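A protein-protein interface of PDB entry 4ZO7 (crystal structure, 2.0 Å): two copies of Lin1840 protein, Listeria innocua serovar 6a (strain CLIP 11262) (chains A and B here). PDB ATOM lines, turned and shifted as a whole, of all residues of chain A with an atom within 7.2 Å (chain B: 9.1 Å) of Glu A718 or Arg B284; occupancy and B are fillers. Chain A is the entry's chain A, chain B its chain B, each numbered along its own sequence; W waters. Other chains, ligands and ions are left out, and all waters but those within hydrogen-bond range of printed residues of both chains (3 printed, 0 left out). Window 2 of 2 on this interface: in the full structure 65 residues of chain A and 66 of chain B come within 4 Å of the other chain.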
ATOM      1  N   PRO A 615     -14.673   9.813   2.082  1.00  0.00           N
ATOM      2  CA  PRO A 615     -15.966   9.354   1.519  1.00  0.00           C
ATOM      3  C   PRO A 615     -16.773  10.439   0.827  1.00  0.00           C
ATOM      4  O   PRO A 615     -16.757  11.624   1.222  1.00  0.00           O
ATOM      5  CB  PRO A 615     -16.753   8.888   2.735  1.00  0.00           C
ATOM      6  CG  PRO A 615     -15.974   9.353   3.953  1.00  0.00           C
ATOM      7  CD  PRO A 615     -14.588   9.704   3.550  1.00  0.00           C
ATOM      8  N   LYS A 616     -17.513  10.017  -0.190  1.00  0.00           N
ATOM      9  CA  LYS A 616     -18.459  10.861  -0.911  1.00  0.00           C
ATOM     10  C   LYS A 616     -19.843  10.948  -0.213  1.00  0.00           C
ATOM     11  O   LYS A 616     -20.624  11.893  -0.432  1.00  0.00           O
ATOM     12  CB  LYS A 616     -18.630  10.330  -2.349  1.00  0.00           C
ATOM     13  CG  LYS A 616     -18.105  11.239  -3.455  1.00  0.00           C
ATOM     14  CD  LYS A 616     -19.182  12.246  -3.918  1.00  0.00           C
ATOM     15  CE  LYS A 616     -19.382  13.449  -2.958  1.00  0.00           C
ATOM     16  NZ  LYS A 616     -20.808  13.798  -2.690  1.00  0.00           N
ATOM     17  N   GLU A 617     -20.157   9.945   0.589  1.00  0.00           N
ATOM     18  CA  GLU A 617     -21.433   9.874   1.278  1.00  0.00           C
ATOM     19  C   GLU A 617     -21.237   9.422   2.702  1.00  0.00           C
ATOM     20  O   GLU A 617     -20.321   8.740   3.010  1.00  0.00           O
ATOM     21  CB  GLU A 617     -22.323   8.871   0.621  1.00  0.00           C
ATOM     22  CG  GLU A 617     -22.638   9.206  -0.801  1.00  0.00           C
ATOM     23  CD  GLU A 617     -23.665   8.238  -1.329  1.00  0.00           C
ATOM     24  OE1 GLU A 617     -24.801   8.692  -1.581  1.00  0.00           O
ATOM     25  OE2 GLU A 617     -23.352   7.009  -1.416  1.00  0.00           O
ATOM     26  N   LEU A 618     -22.118   9.827   3.581  1.00  0.00           N
ATOM     27  CA  LEU A 618     -21.999   9.429   4.959  1.00  0.00           C
ATOM     28  C   LEU A 618     -23.432   9.161   5.437  1.00  0.00           C
ATOM     29  O   LEU A 618     -24.392   9.743   4.900  1.00  0.00           O
ATOM     30  CB  LEU A 618     -21.342  10.595   5.678  1.00  0.00           C
ATOM     31  CG  LEU A 618     -20.593  10.347   6.956  1.00  0.00           C
ATOM     32  CD1 LEU A 618     -19.371   9.455   6.740  1.00  0.00           C
ATOM     33  CD2 LEU A 618     -20.258  11.721   7.507  1.00  0.00           C
ATOM     34  N   ASN A 619     -23.614   8.269   6.392  1.00  0.00           N
ATOM     35  CA  ASN A 619     -24.931   8.066   7.005  1.00  0.00           C
ATOM     36  C   ASN A 619     -25.202   9.106   8.075  1.00  0.00           C
ATOM     37  O   ASN A 619     -24.287   9.691   8.620  1.00  0.00           O
ATOM     38  CB  ASN A 619     -25.084   6.689   7.642  1.00  0.00           C
ATOM     39  CG  ASN A 619     -25.179   5.560   6.614  1.00  0.00           C
ATOM     40  OD1 ASN A 619     -24.462   4.566   6.738  1.00  0.00           O
ATOM     41  ND2 ASN A 619     -26.045   5.704   5.609  1.00  0.00           N
ATOM     42  N   VAL A 649     -24.544  23.322   3.567  1.00  0.00           N
ATOM     43  CA  VAL A 649     -24.829  24.107   2.398  1.00  0.00           C
ATOM     44  C   VAL A 649     -26.285  24.578   2.320  1.00  0.00           C
ATOM     45  O   VAL A 649     -26.565  25.699   1.915  1.00  0.00           O
ATOM     46  CB  VAL A 649     -24.438  23.330   1.130  1.00  0.00           C
ATOM     47  CG1 VAL A 649     -24.780  24.117  -0.094  1.00  0.00           C
ATOM     48  CG2 VAL A 649     -22.947  23.047   1.131  1.00  0.00           C
ATOM     49  N   THR A 650     -27.210  23.704   2.690  1.00  0.00           N
ATOM     50  CA  THR A 650     -28.646  24.016   2.700  1.00  0.00           C
ATOM     51  C   THR A 650     -29.274  23.516   3.963  1.00  0.00           C
ATOM     52  O   THR A 650     -29.041  22.384   4.346  1.00  0.00           O
ATOM     53  CB  THR A 650     -29.337  23.352   1.503  1.00  0.00           C
ATOM     54  OG1 THR A 650     -28.595  23.714   0.329  1.00  0.00           O
ATOM     55  CG2 THR A 650     -30.741  23.830   1.392  1.00  0.00           C
ATOM     56  N   ALA A 651     -30.085  24.356   4.626  1.00  0.00           N
ATOM     57  CA  ALA A 651     -30.714  23.953   5.850  1.00  0.00           C
ATOM     58  C   ALA A 651     -32.026  24.690   6.161  1.00  0.00           C
ATOM     59  O   ALA A 651     -32.404  25.646   5.502  1.00  0.00           O
ATOM     60  CB  ALA A 651     -29.714  24.100   7.006  1.00  0.00           C
ATOM     61  N   PRO A 698     -30.413  15.519   6.682  1.00  0.00           N
ATOM     62  CA  PRO A 698     -29.655  14.974   5.548  1.00  0.00           C
ATOM     63  C   PRO A 698     -29.402  16.086   4.555  1.00  0.00           C
ATOM     64  O   PRO A 698     -30.194  17.033   4.492  1.00  0.00           O
ATOM     65  CB  PRO A 698     -30.562  13.906   4.945  1.00  0.00           C
ATOM     66  CG  PRO A 698     -31.915  14.184   5.460  1.00  0.00           C
ATOM     67  CD  PRO A 698     -31.807  15.035   6.718  1.00  0.00           C
ATOM     68  N   GLY A 699     -28.292  15.954   3.835  1.00  0.00           N
ATOM     69  CA  GLY A 699     -27.911  16.885   2.788  1.00  0.00           C
ATOM     70  C   GLY A 699     -26.415  17.060   2.580  1.00  0.00           C
ATOM     71  O   GLY A 699     -25.605  16.328   3.129  1.00  0.00           O
ATOM     72  N   LEU A 700     -26.064  18.076   1.802  1.00  0.00           N
ATOM     73  CA  LEU A 700     -24.727  18.337   1.398  1.00  0.00           C
ATOM     74  C   LEU A 700     -23.950  19.156   2.446  1.00  0.00           C
ATOM     75  O   LEU A 700     -24.447  20.182   2.912  1.00  0.00           O
ATOM     76  CB  LEU A 700     -24.750  19.130   0.111  1.00  0.00           C
ATOM     77  CG  LEU A 700     -23.351  19.518  -0.402  1.00  0.00           C
ATOM     78  CD1 LEU A 700     -22.484  18.334  -0.812  1.00  0.00           C
ATOM     79  CD2 LEU A 700     -23.526  20.426  -1.606  1.00  0.00           C
ATOM     80  N   HIS A 701     -22.722  18.722   2.751  1.00  0.00           N
ATOM     81  CA  HIS A 701     -21.783  19.512   3.568  1.00  0.00           C
ATOM     82  C   HIS A 701     -20.491  19.627   2.813  1.00  0.00           C
ATOM     83  O   HIS A 701     -20.178  18.755   1.921  1.00  0.00           O
ATOM     84  CB  HIS A 701     -21.491  18.854   4.896  1.00  0.00           C
ATOM     85  CG  HIS A 701     -22.687  18.782   5.804  1.00  0.00           C
ATOM     86  ND1 HIS A 701     -22.848  19.599   6.899  1.00  0.00           N
ATOM     87  CD2 HIS A 701     -23.788  18.000   5.755  1.00  0.00           C
ATOM     88  CE1 HIS A 701     -24.001  19.327   7.477  1.00  0.00           C
ATOM     89  NE2 HIS A 701     -24.575  18.338   6.820  1.00  0.00           N
ATOM     90  N   GLU A 716     -16.581  17.689  -0.621  1.00  0.00           N
ATOM     91  CA  GLU A 716     -18.038  17.572  -0.514  1.00  0.00           C
ATOM     92  C   GLU A 716     -18.413  16.205  -0.017  1.00  0.00           C
ATOM     93  O   GLU A 716     -17.804  15.200  -0.423  1.00  0.00           O
ATOM     94  CB  GLU A 716     -18.718  17.873  -1.843  1.00  0.00           C
ATOM     95  CG  GLU A 716     -18.745  19.381  -2.057  1.00  0.00           C
ATOM     96  CD  GLU A 716     -19.553  19.835  -3.236  1.00  0.00           C
ATOM     97  OE1 GLU A 716     -19.957  18.992  -4.030  1.00  0.00           O
ATOM     98  OE2 GLU A 716     -19.754  21.045  -3.349  1.00  0.00           O
ATOM     99  N   VAL A 717     -19.382  16.181   0.911  1.00  0.00           N
ATOM    100  CA  VAL A 717     -19.909  14.954   1.538  1.00  0.00           C
ATOM    101  C   VAL A 717     -21.397  15.100   1.590  1.00  0.00           C
ATOM    102  O   VAL A 717     -21.915  16.087   2.167  1.00  0.00           O
ATOM    103  CB  VAL A 717     -19.448  14.658   2.998  1.00  0.00           C
ATOM    104  CG1 VAL A 717     -19.976  13.291   3.391  1.00  0.00           C
ATOM    105  CG2 VAL A 717     -17.952  14.563   3.117  1.00  0.00           C
ATOM    106  N   GLU A 718     -22.072  14.098   1.034  1.00  0.00           N
ATOM    107  CA  GLU A 718     -23.500  14.063   1.015  1.00  0.00           C
ATOM    108  C   GLU A 718     -23.930  13.192   2.172  1.00  0.00           C
ATOM    109  O   GLU A 718     -23.617  11.973   2.208  1.00  0.00           O
ATOM    110  CB  GLU A 718     -23.996  13.484  -0.310  1.00  0.00           C
ATOM    111  CG  GLU A 718     -25.499  13.570  -0.497  1.00  0.00           C
ATOM    112  CD  GLU A 718     -26.016  14.988  -0.668  1.00  0.00           C
ATOM    113  OE1 GLU A 718     -27.160  15.246  -0.228  1.00  0.00           O
ATOM    114  OE2 GLU A 718     -25.308  15.831  -1.260  1.00  0.00           O
ATOM    115  N   VAL A 719     -24.658  13.810   3.116  1.00  0.00           N
ATOM    116  CA  VAL A 719     -25.193  13.076   4.280  1.00  0.00           C
ATOM    117  C   VAL A 719     -26.633  12.618   4.066  1.00  0.00           C
ATOM    118  O   VAL A 719     -27.486  13.401   3.681  1.00  0.00           O
ATOM    119  CB  VAL A 719     -25.028  13.815   5.656  1.00  0.00           C
ATOM    120  CG1 VAL A 719     -25.404  12.871   6.784  1.00  0.00           C
ATOM    121  CG2 VAL A 719     -23.600  14.221   5.909  1.00  0.00           C
ATOM    122  N   GLY A 720     -26.885  11.325   4.326  1.00  0.00           N
ATOM    123  CA  GLY A 720     -28.253  10.802   4.357  1.00  0.00           C
ATOM    124  C   GLY A 720     -28.389   9.339   4.703  1.00  0.00           C
ATOM    125  O   GLY A 720     -27.587   8.790   5.449  1.00  0.00           O
ATOM    126  N   GLY A 721     -29.434   8.706   4.184  1.00  0.00           N
ATOM    127  CA  GLY A 721     -29.619   7.266   4.371  1.00  0.00           C
ATOM    128  C   GLY A 721     -30.290   7.044   5.688  1.00  0.00           C
ATOM    129  O   GLY A 721     -31.239   7.744   6.024  1.00  0.00           O
ATOM    130  N   MET B 248     -39.513  33.231   2.915  1.00  0.00           N
ATOM    131  CA  MET B 248     -40.010  31.851   3.109  1.00  0.00           C
ATOM    132  C   MET B 248     -40.287  31.517   4.580  1.00  0.00           C
ATOM    133  O   MET B 248     -40.394  30.334   5.013  1.00  0.00           O
ATOM    134  CB  MET B 248     -39.086  30.857   2.434  1.00  0.00           C
ATOM    135  CG  MET B 248     -37.636  30.822   2.945  1.00  0.00           C
ATOM    136  SD  MET B 248     -36.755  29.301   2.454  1.00  0.00           S
ATOM    137  CE  MET B 248     -37.418  28.291   3.732  1.00  0.00           C
ATOM    138  N   ALA B 275     -35.960  33.619  -5.343  1.00  0.00           N
ATOM    139  CA  ALA B 275     -34.787  32.839  -5.809  1.00  0.00           C
ATOM    140  C   ALA B 275     -33.620  32.937  -4.839  1.00  0.00           C
ATOM    141  O   ALA B 275     -32.861  32.005  -4.670  1.00  0.00           O
ATOM    142  CB  ALA B 275     -34.323  33.316  -7.179  1.00  0.00           C
ATOM    143  N   VAL B 277     -33.463  32.880  -1.674  1.00  0.00           N
ATOM    144  CA  VAL B 277     -33.444  31.989  -0.541  1.00  0.00           C
ATOM    145  C   VAL B 277     -32.468  30.838  -0.776  1.00  0.00           C
ATOM    146  O   VAL B 277     -31.892  30.311   0.208  1.00  0.00           O
ATOM    147  CB  VAL B 277     -34.852  31.516  -0.077  1.00  0.00           C
ATOM    148  CG1 VAL B 277     -35.757  32.697   0.221  1.00  0.00           C
ATOM    149  CG2 VAL B 277     -35.490  30.576  -1.070  1.00  0.00           C
ATOM    150  N   ILE B 278     -32.205  30.529  -2.049  1.00  0.00           N
ATOM    151  CA  ILE B 278     -31.156  29.604  -2.422  1.00  0.00           C
ATOM    152  C   ILE B 278     -29.791  30.143  -1.931  1.00  0.00           C
ATOM    153  O   ILE B 278     -29.035  29.396  -1.281  1.00  0.00           O
ATOM    154  CB  ILE B 278     -31.105  29.300  -3.928  1.00  0.00           C
ATOM    155  CG1 ILE B 278     -32.422  28.735  -4.432  1.00  0.00           C
ATOM    156  CG2 ILE B 278     -30.032  28.258  -4.208  1.00  0.00           C
ATOM    157  CD1 ILE B 278     -32.609  28.789  -5.935  1.00  0.00           C
ATOM    158  N   ASN B 279     -29.498  31.417  -2.197  1.00  0.00           N
ATOM    159  CA  ASN B 279     -28.242  31.976  -1.800  1.00  0.00           C
ATOM    160  C   ASN B 279     -28.038  31.950  -0.291  1.00  0.00           C
ATOM    161  O   ASN B 279     -26.929  31.708   0.202  1.00  0.00           O
ATOM    162  CB  ASN B 279     -28.071  33.402  -2.290  1.00  0.00           C
ATOM    163  CG  ASN B 279     -27.863  33.495  -3.774  1.00  0.00           C
ATOM    164  OD1 ASN B 279     -27.347  32.567  -4.401  1.00  0.00           O
ATOM    165  ND2 ASN B 279     -28.261  34.618  -4.351  1.00  0.00           N
ATOM    166  N   HIS B 280     -29.111  32.241   0.418  1.00  0.00           N
ATOM    167  CA  HIS B 280     -29.149  32.200   1.864  1.00  0.00           C
ATOM    168  C   HIS B 280     -28.963  30.784   2.406  1.00  0.00           C
ATOM    169  O   HIS B 280     -28.730  30.609   3.578  1.00  0.00           O
ATOM    170  CB  HIS B 280     -30.526  32.631   2.356  1.00  0.00           C
ATOM    171  CG  HIS B 280     -30.747  34.097   2.525  1.00  0.00           C
ATOM    172  ND1 HIS B 280     -30.113  34.836   3.497  1.00  0.00           N
ATOM    173  CD2 HIS B 280     -31.713  34.899   2.013  1.00  0.00           C
ATOM    174  CE1 HIS B 280     -30.634  36.049   3.533  1.00  0.00           C
ATOM    175  NE2 HIS B 280     -31.607  36.116   2.636  1.00  0.00           N
ATOM    176  N   GLY B 281     -29.085  29.762   1.575  1.00  0.00           N
ATOM    177  CA  GLY B 281     -28.827  28.398   2.044  1.00  0.00           C
ATOM    178  C   GLY B 281     -29.984  27.721   2.751  1.00  0.00           C
ATOM    179  O   GLY B 281     -29.782  26.788   3.496  1.00  0.00           O
ATOM    180  N   THR B 282     -31.195  28.209   2.538  1.00  0.00           N
ATOM    181  CA  THR B 282     -32.405  27.602   3.033  1.00  0.00           C
ATOM    182  C   THR B 282     -33.279  26.953   1.918  1.00  0.00           C
ATOM    183  O   THR B 282     -34.379  26.473   2.194  1.00  0.00           O
ATOM    184  CB  THR B 282     -33.265  28.590   3.913  1.00  0.00           C
ATOM    185  OG1 THR B 282     -33.666  29.738   3.150  1.00  0.00           O
ATOM    186  CG2 THR B 282     -32.475  29.090   5.192  1.00  0.00           C
ATOM    187  N   ALA B 283     -32.820  26.952   0.681  1.00  0.00           N
ATOM    188  CA  ALA B 283     -33.441  26.093  -0.373  1.00  0.00           C
ATOM    189  C   ALA B 283     -32.310  25.546  -1.219  1.00  0.00           C
ATOM    190  O   ALA B 283     -31.332  26.250  -1.441  1.00  0.00           O
ATOM    191  CB  ALA B 283     -34.397  26.863  -1.220  1.00  0.00           C
ATOM    192  N   ARG B 284     -32.418  24.297  -1.647  1.00  0.00           N
ATOM    193  CA  ARG B 284     -31.388  23.705  -2.502  1.00  0.00           C
ATOM    194  C   ARG B 284     -31.457  24.191  -3.963  1.00  0.00           C
ATOM    195  O   ARG B 284     -30.464  24.224  -4.649  1.00  0.00           O
ATOM    196  CB  ARG B 284     -31.444  22.150  -2.416  1.00  0.00           C
ATOM    197  CG  ARG B 284     -30.226  21.424  -2.954  1.00  0.00           C
ATOM    198  CD  ARG B 284     -30.132  19.966  -2.490  1.00  0.00           C
ATOM    199  NE  ARG B 284     -28.830  19.380  -2.837  1.00  0.00           N
ATOM    200  CZ  ARG B 284     -28.246  18.301  -2.270  1.00  0.00           C
ATOM    201  NH1 ARG B 284     -27.054  17.894  -2.699  1.00  0.00           N
ATOM    202  NH2 ARG B 284     -28.813  17.628  -1.268  1.00  0.00           N
ATOM    203  N   ASN B 285     -32.618  24.569  -4.453  1.00  0.00           N
ATOM    204  CA  ASN B 285     -32.798  24.862  -5.891  1.00  0.00           C
ATOM    205  C   ASN B 285     -34.085  25.630  -6.131  1.00  0.00           C
ATOM    206  O   ASN B 285     -34.814  25.896  -5.161  1.00  0.00           O
ATOM    207  CB  ASN B 285     -32.800  23.557  -6.698  1.00  0.00           C
ATOM    208  CG  ASN B 285     -33.723  22.508  -6.098  1.00  0.00           C
ATOM    209  OD1 ASN B 285     -34.788  22.813  -5.579  1.00  0.00           O
ATOM    210  ND2 ASN B 285     -33.314  21.250  -6.177  1.00  0.00           N
ATOM    211  N   PRO B 286     -34.371  26.003  -7.404  1.00  0.00           N
ATOM    212  CA  PRO B 286     -35.591  26.770  -7.593  1.00  0.00           C
ATOM    213  C   PRO B 286     -36.874  26.035  -7.203  1.00  0.00           C
ATOM    214  O   PRO B 286     -37.824  26.654  -6.756  1.00  0.00           O
ATOM    215  CB  PRO B 286     -35.559  27.104  -9.077  1.00  0.00           C
ATOM    216  CG  PRO B 286     -34.127  27.330  -9.307  1.00  0.00           C
ATOM    217  CD  PRO B 286     -33.423  26.252  -8.506  1.00  0.00           C
ATOM    218  N   LYS B 287     -36.881  24.718  -7.300  1.00  0.00           N
ATOM    219  CA  LYS B 287     -38.101  23.970  -6.937  1.00  0.00           C
ATOM    220  C   LYS B 287     -38.414  24.130  -5.437  1.00  0.00           C
ATOM    221  O   LYS B 287     -39.545  24.388  -5.055  1.00  0.00           O
ATOM    222  CB  LYS B 287     -37.936  22.497  -7.317  1.00  0.00           C
ATOM    223  CG  LYS B 287     -39.151  21.630  -7.112  1.00  0.00           C
ATOM    224  CD  LYS B 287     -38.818  20.164  -7.362  1.00  0.00           C
ATOM    225  CE  LYS B 287     -40.065  19.340  -7.674  1.00  0.00           C
ATOM    226  NZ  LYS B 287     -39.682  18.038  -8.254  1.00  0.00           N
ATOM    227  N   GLU B 288     -37.410  23.953  -4.594  1.00  0.00           N
ATOM    228  CA  GLU B 288     -37.605  24.186  -3.145  1.00  0.00           C
ATOM    229  C   GLU B 288     -37.930  25.647  -2.869  1.00  0.00           C
ATOM    230  O   GLU B 288     -38.787  25.926  -2.025  1.00  0.00           O
ATOM    231  CB  GLU B 288     -36.352  23.775  -2.325  1.00  0.00           C
ATOM    232  CG  GLU B 288     -36.034  22.303  -2.439  1.00  0.00           C
ATOM    233  CD  GLU B 288     -35.093  21.765  -1.374  1.00  0.00           C
ATOM    234  OE1 GLU B 288     -34.419  22.529  -0.643  1.00  0.00           O
ATOM    235  OE2 GLU B 288     -34.986  20.535  -1.332  1.00  0.00           O
ATOM    236  N   ALA B 289     -37.245  26.593  -3.535  1.00  0.00           N
ATOM    237  CA  ALA B 289     -37.531  28.032  -3.280  1.00  0.00           C
ATOM    238  C   ALA B 289     -39.008  28.331  -3.512  1.00  0.00           C
ATOM    239  O   ALA B 289     -39.675  29.028  -2.711  1.00  0.00           O
ATOM    240  CB  ALA B 289     -36.667  28.935  -4.167  1.00  0.00           C
ATOM    241  N   ALA B 290     -39.510  27.807  -4.631  1.00  0.00           N
ATOM    242  CA  ALA B 290     -40.914  27.975  -5.017  1.00  0.00           C
ATOM    243  C   ALA B 290     -41.824  27.343  -3.948  1.00  0.00           C
ATOM    244  O   ALA B 290     -42.766  27.929  -3.464  1.00  0.00           O
ATOM    245  CB  ALA B 290     -41.154  27.296  -6.394  1.00  0.00           C
ATOM    246  N   PHE B 292     -41.299  26.491  -0.826  1.00  0.00           N
ATOM    247  CA  PHE B 292     -41.274  27.141   0.499  1.00  0.00           C
ATOM    248  C   PHE B 292     -41.864  28.558   0.454  1.00  0.00           C
ATOM    249  O   PHE B 292     -42.600  28.979   1.353  1.00  0.00           O
ATOM    250  CB  PHE B 292     -39.856  27.122   1.075  1.00  0.00           C
ATOM    251  CG  PHE B 292     -39.241  25.775   1.131  1.00  0.00           C
ATOM    252  CD1 PHE B 292     -40.015  24.634   1.305  1.00  0.00           C
ATOM    253  CD2 PHE B 292     -37.851  25.650   1.096  1.00  0.00           C
ATOM    254  CE1 PHE B 292     -39.414  23.388   1.439  1.00  0.00           C
ATOM    255  CE2 PHE B 292     -37.241  24.411   1.203  1.00  0.00           C
ATOM    256  CZ  PHE B 292     -38.022  23.275   1.382  1.00  0.00           C
HETATM  257  O   HOH W   1     -35.394  24.875   4.294  1.00  0.00           O
HETATM  258  O   HOH W   2     -28.635  26.182  -0.873  1.00  0.00           O
HETATM  259  O   HOH W   3     -28.175  20.048   0.804  1.00  0.00           O
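The side-chain carboxylate (OE2) of Glu A718 is in salt-bridge range of the guanidinium group (NH1) of Arg B284 (3.1 Å). O of Gly B281 is in hydrogen-bond range of N of Ala A651, at 2.7 Å.
No position is printed for both chains. Of the 8 pairs that touch across the chains among the printed residues, none has its exchanged pair printed and touching as well.
N of Arg B284 lies within hydrogen-bond range of OE1 of Glu B288, at 2.9 Å. N of Thr B282 is in hydrogen-bond range of O of Val B277 (3.2 Å). The backbone NH of Leu A618 sits at hydrogen-bond distance from the backbone carbonyl oxygen of Glu A718, at 3.0 Å. N of Val A649 lies within hydrogen-bond range of O of Leu A700, 3.2 Å away. The side-chain hydroxyl (OG1) of Thr B282 is in hydrogen-bond range of the side-chain sulfur (SD) of Met B248 (3.2 Å). O of Lys A616 is in hydrogen-bond range of N of Glu A718.
Of the printed residues of chain B, Ala A651 touches Gly B281 and Thr B282. His A701 touches none of the printed residues of chain B. No residue of chain B comes within 4 Å of Val A717. Glu A718 touches just one residue of chain B: Arg B284 (3.1 Å). No residue of chain B comes within 4 Å of Val A719. Of the printed residues of chain A, Gly B281 touches Val A649, Thr A650 and Ala A651. Printed residues of chain A within 4 Å of Arg B284: Thr A650 (3.5 Å), Leu A700 (3.8 Å) and Glu A718 (3.1 Å). Glu B288 touches none of the printed residues of chain A. The nearest printed residue of chain A that does not touch Gly B281 is Leu A700 (8.5 Å).
Of the 17 printed residues of chain B, 4 touch a printed residue of chain A. Printed residues of chain A that touch a printed residue of chain B: Val A649, Thr A650, Ala A651, Leu A700 and Glu A718. Hydrophobic or aromatic side chains of chain A that line the printed part of chain B: Leu A700. Among the printed residues, 8 pairs touch across the chains. Among the printed residues, Asp or Glu carboxylates within 4 Å of a Lys or Arg side-chain nitrogen of the other chain: Glu A718 with Arg B284 (3.1 Å).
Water W2 lies within hydrogen-bond range of the side-chain hydroxyl of Thr A650 (2.7 Å), the backbone carbonyl oxygen of Ala B283 (2.8 Å) and the backbone carbonyl oxygen of Ile B278 (3.3 Å). Water W1 lies within hydrogen-bond range of O of Thr B282 (2.8 Å) and O of Ala A651 (3.3 Å). Water W3 bridges N of Leu A700 (3.1 Å) and NH2 of Arg B284 (3.2 Å).
Among the printed residues, merely in contact across the chains: Val A649 with Gly B281 (3.5 Å), Thr A650 with Gly B281 (3.1 Å), Thr A650 with Ala B283 (3.5 Å), Thr A650 with Arg B284 (3.5 Å), Ala A651 with Thr B282 (3.1 Å) and Leu A700 with Arg B284 (3.8 Å).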
